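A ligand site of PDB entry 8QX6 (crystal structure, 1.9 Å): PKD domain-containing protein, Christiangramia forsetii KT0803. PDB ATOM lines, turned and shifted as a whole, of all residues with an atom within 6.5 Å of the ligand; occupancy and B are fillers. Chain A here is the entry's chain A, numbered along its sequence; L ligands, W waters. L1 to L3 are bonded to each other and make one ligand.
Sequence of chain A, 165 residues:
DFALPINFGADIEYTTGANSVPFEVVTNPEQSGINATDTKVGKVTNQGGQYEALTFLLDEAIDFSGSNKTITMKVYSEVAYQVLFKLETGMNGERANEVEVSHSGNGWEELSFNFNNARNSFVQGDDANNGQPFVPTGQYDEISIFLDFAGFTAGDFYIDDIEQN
Water W2 lies within hydrogen-bond range of an oxygen (O1) of LIG L1 (2.5 Å), the backbone NH (N) of Ala 53 (2.9 Å) and the backbone carbonyl oxygen (O) of Asn 19 (2.9 Å).
Water W5 lies within hydrogen-bond range of O5 of LIG L1 (2.8 Å), OG1 of Thr 55 (3.1 Å) and O of Asn 19 (3.3 Å).
Water W3 bridges OH of Tyr 51 and O3 of LG3 L3.
Water W1 lies within hydrogen-bond range of the side-chain carboxylate (OE2) of Glu 98, the backbone NH (N) of Phe 122 and an oxygen (O5) of LG3 L3.
Water W4 bridges the backbone NH of Asn 19 and an oxygen (O6) of LIG L1.
The backbone carbonyl oxygen (O) of Leu 84 sits at hydrogen-bond distance from the backbone NH (N) of Phe 146 (2.9 Å).
OE2 of Glu 88 lies within salt-bridge range of NZ of Lys 86 (3.9 Å).
The backbone NH (N) of Glu 88 is in hydrogen-bond range of the backbone carbonyl oxygen (O) of Glu 142 (3.0 Å).
N of Lys 86 lies within hydrogen-bond range of O of Ser 144 (2.7 Å).
The side-chain carboxylate (OE1) of Glu 88 sits at hydrogen-bond distance from the side-chain hydroxyl (OG) of Ser 144 (2.5 Å).
NH2 of Arg 119 lies within salt-bridge range of OE2 of Glu 98 (3.1 Å).
The side-chain carboxylate (OE1) of Glu 98 sits at hydrogen-bond distance from the side-chain hydroxyl (OG) of Ser 121 (2.5 Å).
CD2 of Leu 84 touches C5 of LG2 L2 (3.4 Å).
Ser 121 touches the ligand.
CD2 of Phe 122 touches C1 of LG3 L3, at 3.4 Å.
CZ of Phe 146 touches O4 of LG2 L2 (3.4 Å).
Phe 149 touches the ligand.
Of the 19 residues printed, 9 come within 4 Å of the ligand.
OE2 of Glu 88 is in hydrogen-bond range of O4 of LIG L1 (2.5 Å).
O of Tyr 51 is in hydrogen-bond range of O2 of LIG L1.
OE1 of Glu 98 lies within hydrogen-bond range of O5 of LG2 L2, 2.6 Å away.
The side-chain amino group (NZ) of Lys 86 lies within hydrogen-bond range of an oxygen (O4) of LIG L1 (2.8 Å).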
ATOM      1  N   ASN A  19     -13.916  15.441  29.715  1.00  0.00           N
ATOM      2  CA  ASN A  19     -12.926  15.803  28.665  1.00  0.00           C
ATOM      3  C   ASN A  19     -13.461  16.942  27.786  1.00  0.00           C
ATOM      4  O   ASN A  19     -12.784  17.285  26.805  1.00  0.00           O
ATOM      5  CB  ASN A  19     -12.513  14.570  27.860  1.00  0.00           C
ATOM      6  CG  ASN A  19     -11.663  13.641  28.702  1.00  0.00           C
ATOM      7  OD1 ASN A  19     -10.575  14.014  29.129  1.00  0.00           O
ATOM      8  ND2 ASN A  19     -12.169  12.446  28.973  1.00  0.00           N
ATOM      9  N   SER A  20     -14.575  17.551  28.149  1.00  0.00           N
ATOM     10  CA  SER A  20     -15.205  18.642  27.370  1.00  0.00           C
ATOM     11  C   SER A  20     -14.201  19.778  27.209  1.00  0.00           C
ATOM     12  O   SER A  20     -13.477  20.102  28.160  1.00  0.00           O
ATOM     13  CB  SER A  20     -16.474  19.129  28.002  1.00  0.00           C
ATOM     14  OG  SER A  20     -17.094  20.092  27.177  1.00  0.00           O
ATOM     15  N   TYR A  51      -9.894  16.084  17.592  1.00  0.00           N
ATOM     16  CA  TYR A  51     -11.260  15.548  17.818  1.00  0.00           C
ATOM     17  C   TYR A  51     -11.786  16.083  19.151  1.00  0.00           C
ATOM     18  O   TYR A  51     -12.493  15.384  19.879  1.00  0.00           O
ATOM     19  CB  TYR A  51     -11.204  14.020  17.718  1.00  0.00           C
ATOM     20  CG  TYR A  51     -10.779  13.555  16.348  1.00  0.00           C
ATOM     21  CD1 TYR A  51     -11.569  13.818  15.238  1.00  0.00           C
ATOM     22  CD2 TYR A  51      -9.617  12.812  16.141  1.00  0.00           C
ATOM     23  CE1 TYR A  51     -11.225  13.388  13.975  1.00  0.00           C
ATOM     24  CE2 TYR A  51      -9.244  12.388  14.876  1.00  0.00           C
ATOM     25  CZ  TYR A  51     -10.049  12.671  13.788  1.00  0.00           C
ATOM     26  OH  TYR A  51      -9.685  12.288  12.536  1.00  0.00           O
ATOM     27  N   GLU A  52     -11.418  17.323  19.489  1.00  0.00           N
ATOM     28  CA  GLU A  52     -11.897  17.968  20.739  1.00  0.00           C
ATOM     29  C   GLU A  52     -13.396  18.234  20.563  1.00  0.00           C
ATOM     30  O   GLU A  52     -13.809  18.669  19.465  1.00  0.00           O
ATOM     31  CB  GLU A  52     -11.085  19.221  21.096  1.00  0.00           C
ATOM     32  CG  GLU A  52     -11.349  20.447  20.237  1.00  0.00           C
ATOM     33  CD  GLU A  52     -10.395  21.611  20.473  1.00  0.00           C
ATOM     34  OE1 GLU A  52      -9.924  21.767  21.601  1.00  0.00           O
ATOM     35  OE2 GLU A  52     -10.110  22.342  19.531  1.00  0.00           O
ATOM     36  N   ALA A  53     -14.172  17.896  21.592  1.00  0.00           N
ATOM     37  CA  ALA A  53     -15.660  17.946  21.627  1.00  0.00           C
ATOM     38  C   ALA A  53     -16.121  18.724  22.853  1.00  0.00           C
ATOM     39  O   ALA A  53     -15.502  18.585  23.964  1.00  0.00           O
ATOM     40  CB  ALA A  53     -16.215  16.570  21.646  1.00  0.00           C
ATOM     41  N   THR A  55     -18.973  18.233  25.276  1.00  0.00           N
ATOM     42  CA  THR A  55     -19.789  17.059  25.688  1.00  0.00           C
ATOM     43  C   THR A  55     -20.733  17.471  26.828  1.00  0.00           C
ATOM     44  O   THR A  55     -20.238  17.993  27.814  1.00  0.00           O
ATOM     45  CB  THR A  55     -18.921  15.846  26.048  1.00  0.00           C
ATOM     46  OG1 THR A  55     -18.195  15.531  24.861  1.00  0.00           O
ATOM     47  CG2 THR A  55     -19.727  14.649  26.511  1.00  0.00           C
ATOM     48  N   LEU A  84     -19.578  18.248  13.704  1.00  0.00           N
ATOM     49  CA  LEU A  84     -20.130  16.896  14.017  1.00  0.00           C
ATOM     50  C   LEU A  84     -21.070  17.020  15.200  1.00  0.00           C
ATOM     51  O   LEU A  84     -20.688  17.663  16.202  1.00  0.00           O
ATOM     52  CB  LEU A  84     -19.002  15.889  14.321  1.00  0.00           C
ATOM     53  CG  LEU A  84     -19.452  14.432  14.306  1.00  0.00           C
ATOM     54  CD1 LEU A  84     -19.752  13.990  12.888  1.00  0.00           C
ATOM     55  CD2 LEU A  84     -18.394  13.509  14.914  1.00  0.00           C
ATOM     56  N   LYS A  86     -22.749  14.312  17.646  1.00  0.00           N
ATOM     57  CA  LYS A  86     -22.506  12.904  18.020  1.00  0.00           C
ATOM     58  C   LYS A  86     -23.382  12.543  19.214  1.00  0.00           C
ATOM     59  O   LYS A  86     -23.351  13.274  20.224  1.00  0.00           O
ATOM     60  CB  LYS A  86     -21.037  12.664  18.353  1.00  0.00           C
ATOM     61  CG  LYS A  86     -20.743  11.368  19.079  1.00  0.00           C
ATOM     62  CD  LYS A  86     -19.241  11.062  19.124  1.00  0.00           C
ATOM     63  CE  LYS A  86     -18.940   9.622  19.454  1.00  0.00           C
ATOM     64  NZ  LYS A  86     -17.480   9.389  19.532  1.00  0.00           N
ATOM     65  N   GLU A  88     -23.232   9.828  21.936  1.00  0.00           N
ATOM     66  CA  GLU A  88     -22.363   8.781  22.542  1.00  0.00           C
ATOM     67  C   GLU A  88     -23.289   7.635  22.951  1.00  0.00           C
ATOM     68  O   GLU A  88     -24.523   7.846  22.933  1.00  0.00           O
ATOM     69  CB  GLU A  88     -21.480   9.289  23.700  1.00  0.00           C
ATOM     70  CG  GLU A  88     -20.023   9.602  23.283  1.00  0.00           C
ATOM     71  CD  GLU A  88     -19.854  11.083  23.052  1.00  0.00           C
ATOM     72  OE1 GLU A  88     -20.738  11.802  23.536  1.00  0.00           O
ATOM     73  OE2 GLU A  88     -18.853  11.531  22.424  1.00  0.00           O
ATOM     74  N   GLU A  98     -23.502   9.611  14.636  1.00  0.00           N
ATOM     75  CA  GLU A  98     -23.140  11.028  14.382  1.00  0.00           C
ATOM     76  C   GLU A  98     -23.578  11.461  12.990  1.00  0.00           C
ATOM     77  O   GLU A  98     -23.706  10.603  12.087  1.00  0.00           O
ATOM     78  CB  GLU A  98     -21.637  11.247  14.540  1.00  0.00           C
ATOM     79  CG  GLU A  98     -20.817  10.382  13.601  1.00  0.00           C
ATOM     80  CD  GLU A  98     -19.382  10.155  14.045  1.00  0.00           C
ATOM     81  OE1 GLU A  98     -19.169  10.034  15.259  1.00  0.00           O
ATOM     82  OE2 GLU A  98     -18.490  10.172  13.186  1.00  0.00           O
ATOM     83  N   ARG A 119     -24.267   7.995  10.789  1.00  0.00           N
ATOM     84  CA  ARG A 119     -23.315   6.865  10.611  1.00  0.00           C
ATOM     85  C   ARG A 119     -22.819   6.446  12.001  1.00  0.00           C
ATOM     86  O   ARG A 119     -22.874   7.262  12.998  1.00  0.00           O
ATOM     87  CB  ARG A 119     -22.155   7.320   9.725  1.00  0.00           C
ATOM     88  CG  ARG A 119     -21.211   8.312  10.401  1.00  0.00           C
ATOM     89  CD  ARG A 119     -20.275   9.013   9.422  1.00  0.00           C
ATOM     90  NE  ARG A 119     -19.424   9.901  10.182  1.00  0.00           N
ATOM     91  CZ  ARG A 119     -18.839  11.008   9.737  1.00  0.00           C
ATOM     92  NH1 ARG A 119     -19.019  11.398   8.492  1.00  0.00           N
ATOM     93  NH2 ARG A 119     -18.097  11.742  10.551  1.00  0.00           N
ATOM     94  N   SER A 121     -20.338   6.035  14.748  1.00  0.00           N
ATOM     95  CA  SER A 121     -19.164   6.729  15.317  1.00  0.00           C
ATOM     96  C   SER A 121     -17.991   5.762  15.377  1.00  0.00           C
ATOM     97  O   SER A 121     -18.196   4.572  15.636  1.00  0.00           O
ATOM     98  CB  SER A 121     -19.487   7.318  16.631  1.00  0.00           C
ATOM     99  OG  SER A 121     -20.493   8.324  16.491  1.00  0.00           O
ATOM    100  N   PHE A 122     -16.785   6.263  15.128  1.00  0.00           N
ATOM    101  CA  PHE A 122     -15.521   5.496  15.287  1.00  0.00           C
ATOM    102  C   PHE A 122     -15.476   4.875  16.687  1.00  0.00           C
ATOM    103  O   PHE A 122     -15.667   5.574  17.687  1.00  0.00           O
ATOM    104  CB  PHE A 122     -14.277   6.337  14.998  1.00  0.00           C
ATOM    105  CG  PHE A 122     -13.018   5.512  15.067  1.00  0.00           C
ATOM    106  CD1 PHE A 122     -12.549   4.854  13.941  1.00  0.00           C
ATOM    107  CD2 PHE A 122     -12.368   5.300  16.265  1.00  0.00           C
ATOM    108  CE1 PHE A 122     -11.442   4.018  14.001  1.00  0.00           C
ATOM    109  CE2 PHE A 122     -11.260   4.473  16.335  1.00  0.00           C
ATOM    110  CZ  PHE A 122     -10.797   3.837  15.208  1.00  0.00           C
ATOM    111  N   VAL A 123     -15.335   3.552  16.733  1.00  0.00           N
ATOM    112  CA  VAL A 123     -14.979   2.818  17.973  1.00  0.00           C
ATOM    113  C   VAL A 123     -13.790   1.919  17.616  1.00  0.00           C
ATOM    114  O   VAL A 123     -13.830   1.190  16.586  1.00  0.00           O
ATOM    115  CB  VAL A 123     -16.168   2.043  18.609  1.00  0.00           C
ATOM    116  CG1 VAL A 123     -17.494   2.804  18.631  1.00  0.00           C
ATOM    117  CG2 VAL A 123     -16.358   0.691  18.000  1.00  0.00           C
ATOM    118  N   GLN A 124     -12.733   2.003  18.421  1.00  0.00           N
ATOM    119  CA  GLN A 124     -11.510   1.170  18.264  1.00  0.00           C
ATOM    120  C   GLN A 124     -11.936  -0.292  18.201  1.00  0.00           C
ATOM    121  O   GLN A 124     -12.698  -0.724  19.061  1.00  0.00           O
ATOM    122  CB  GLN A 124     -10.522   1.422  19.420  1.00  0.00           C
ATOM    123  CG  GLN A 124      -9.620   2.627  19.156  1.00  0.00           C
ATOM    124  CD  GLN A 124      -8.423   2.698  20.085  1.00  0.00           C
ATOM    125  OE1 GLN A 124      -8.168   3.721  20.719  1.00  0.00           O
ATOM    126  NE2 GLN A 124      -7.682   1.602  20.158  1.00  0.00           N
ATOM    127  N   GLU A 142     -26.094  11.492  26.404  1.00  0.00           N
ATOM    128  CA  GLU A 142     -24.764  12.142  26.251  1.00  0.00           C
ATOM    129  C   GLU A 142     -24.537  12.556  24.781  1.00  0.00           C
ATOM    130  O   GLU A 142     -24.497  11.685  23.880  1.00  0.00           O
ATOM    131  CB  GLU A 142     -23.690  11.216  26.791  1.00  0.00           C
ATOM    132  CG  GLU A 142     -22.353  11.916  26.976  1.00  0.00           C
ATOM    133  CD  GLU A 142     -21.310  11.081  27.699  1.00  0.00           C
ATOM    134  OE1 GLU A 142     -21.710  10.206  28.509  1.00  0.00           O
ATOM    135  OE2 GLU A 142     -20.126  11.310  27.470  1.00  0.00           O
ATOM    136  N   SER A 144     -22.210  15.058  21.977  1.00  0.00           N
ATOM    137  CA  SER A 144     -20.882  15.644  21.717  1.00  0.00           C
ATOM    138  C   SER A 144     -20.951  16.461  20.427  1.00  0.00           C
ATOM    139  O   SER A 144     -21.333  15.905  19.362  1.00  0.00           O
ATOM    140  CB  SER A 144     -19.802  14.586  21.679  1.00  0.00           C
ATOM    141  OG  SER A 144     -19.630  13.992  22.956  1.00  0.00           O
ATOM    142  N   PHE A 146     -18.585  18.695  17.890  1.00  0.00           N
ATOM    143  CA  PHE A 146     -17.209  18.908  17.394  1.00  0.00           C
ATOM    144  C   PHE A 146     -17.223  20.109  16.437  1.00  0.00           C
ATOM    145  O   PHE A 146     -17.810  19.984  15.352  1.00  0.00           O
ATOM    146  CB  PHE A 146     -16.661  17.657  16.719  1.00  0.00           C
ATOM    147  CG  PHE A 146     -16.604  16.403  17.553  1.00  0.00           C
ATOM    148  CD1 PHE A 146     -17.763  15.757  17.949  1.00  0.00           C
ATOM    149  CD2 PHE A 146     -15.395  15.808  17.871  1.00  0.00           C
ATOM    150  CE1 PHE A 146     -17.711  14.601  18.709  1.00  0.00           C
ATOM    151  CE2 PHE A 146     -15.350  14.616  18.576  1.00  0.00           C
ATOM    152  CZ  PHE A 146     -16.505  14.013  18.999  1.00  0.00           C
ATOM    153  N   PHE A 149     -14.435  19.535  13.216  1.00  0.00           N
ATOM    154  CA  PHE A 149     -14.270  18.070  13.249  1.00  0.00           C
ATOM    155  C   PHE A 149     -13.071  17.670  12.382  1.00  0.00           C
ATOM    156  O   PHE A 149     -13.044  17.993  11.186  1.00  0.00           O
ATOM    157  CB  PHE A 149     -15.552  17.340  12.828  1.00  0.00           C
ATOM    158  CG  PHE A 149     -15.361  15.850  12.733  1.00  0.00           C
ATOM    159  CD1 PHE A 149     -15.107  15.106  13.877  1.00  0.00           C
ATOM    160  CD2 PHE A 149     -15.332  15.209  11.507  1.00  0.00           C
ATOM    161  CE1 PHE A 149     -14.854  13.741  13.790  1.00  0.00           C
ATOM    162  CE2 PHE A 149     -15.089  13.847  11.429  1.00  0.00           C
ATOM    163  CZ  PHE A 149     -14.848  13.109  12.569  1.00  0.00           C
HETATM  164  C1  LIG L   1     -13.056  12.443  22.001  1.00  0.00           C
HETATM  165  C2  LIG L   1     -14.260  11.914  21.224  1.00  0.00           C
HETATM  166  C3  LIG L   1     -15.372  11.505  22.177  1.00  0.00           C
HETATM  167  C4  LIG L   1     -15.632  12.567  23.257  1.00  0.00           C
HETATM  168  C5  LIG L   1     -16.351  11.883  24.419  1.00  0.00           C
HETATM  169  C6  LIG L   1     -13.543  13.692  22.758  1.00  0.00           C
HETATM  170  O1  LIG L   1     -12.452  14.444  23.292  1.00  0.00           O
HETATM  171  O2  LIG L   1     -12.012  12.754  21.093  1.00  0.00           O
HETATM  172  O3  LIG L   1     -13.854  10.747  20.505  1.00  0.00           O
HETATM  173  O4  LIG L   1     -16.579  11.202  21.427  1.00  0.00           O
HETATM  174  O5  LIG L   1     -14.436  13.196  23.769  1.00  0.00           O
HETATM  175  O6  LIG L   1     -15.564  11.839  25.613  1.00  0.00           O
HETATM  176  C1  LG2 L   2     -12.877   9.829  18.583  1.00  0.00           C
HETATM  177  C2  LG2 L   2     -12.693   9.983  17.095  1.00  0.00           C
HETATM  178  C3  LG2 L   2     -14.075  10.056  16.477  1.00  0.00           C
HETATM  179  C4  LG2 L   2     -14.850  11.225  17.062  1.00  0.00           C
HETATM  180  C5  LG2 L   2     -16.262  11.301  16.485  1.00  0.00           C
HETATM  181  C6  LG2 L   2     -13.673  10.996  19.133  1.00  0.00           C
HETATM  182  O1  LG2 L   2     -11.608   9.751  19.182  1.00  0.00           O
HETATM  183  O2  LG2 L   2     -11.947   8.822  16.685  1.00  0.00           O
HETATM  184  O3  LG2 L   2     -13.896  10.282  15.098  1.00  0.00           O
HETATM  185  O4  LG2 L   2     -14.938  11.050  18.468  1.00  0.00           O
HETATM  186  O5  LG2 L   2     -17.012  10.114  16.701  1.00  0.00           O
HETATM  187  C1  LG3 L   3     -10.196   7.820  15.511  1.00  0.00           C
HETATM  188  C2  LG3 L   3      -9.231   7.878  14.355  1.00  0.00           C
HETATM  189  C3  LG3 L   3     -10.076   7.942  13.098  1.00  0.00           C
HETATM  190  C4  LG3 L   3     -11.192   9.029  13.162  1.00  0.00           C
HETATM  191  C5  LG3 L   3     -12.240   8.957  12.056  1.00  0.00           C
HETATM  192  C6  LG3 L   3     -11.152   9.004  15.528  1.00  0.00           C
HETATM  193  O1  LG3 L   3      -9.510   7.797  16.737  1.00  0.00           O
HETATM  194  O2  LG3 L   3      -8.388   6.698  14.358  1.00  0.00           O
HETATM  195  O3  LG3 L   3      -9.177   8.226  12.027  1.00  0.00           O
HETATM  196  O4  LG3 L   3     -11.940   8.915  14.355  1.00  0.00           O
HETATM  197  O5  LG3 L   3     -13.546   8.834  12.644  1.00  0.00           O
HETATM  198  O   HOH W   1     -16.393   8.880  13.824  1.00  0.00           O
HETATM  199  O   HOH W   2     -12.946  16.799  23.951  1.00  0.00           O
HETATM  200  O   HOH W   3      -7.779  10.912  12.046  1.00  0.00           O
HETATM  201  O   HOH W   4     -16.014  14.308  28.035  1.00  0.00           O
HETATM  202  O   HOH W   5     -15.157  15.381  25.449  1.00  0.00           O
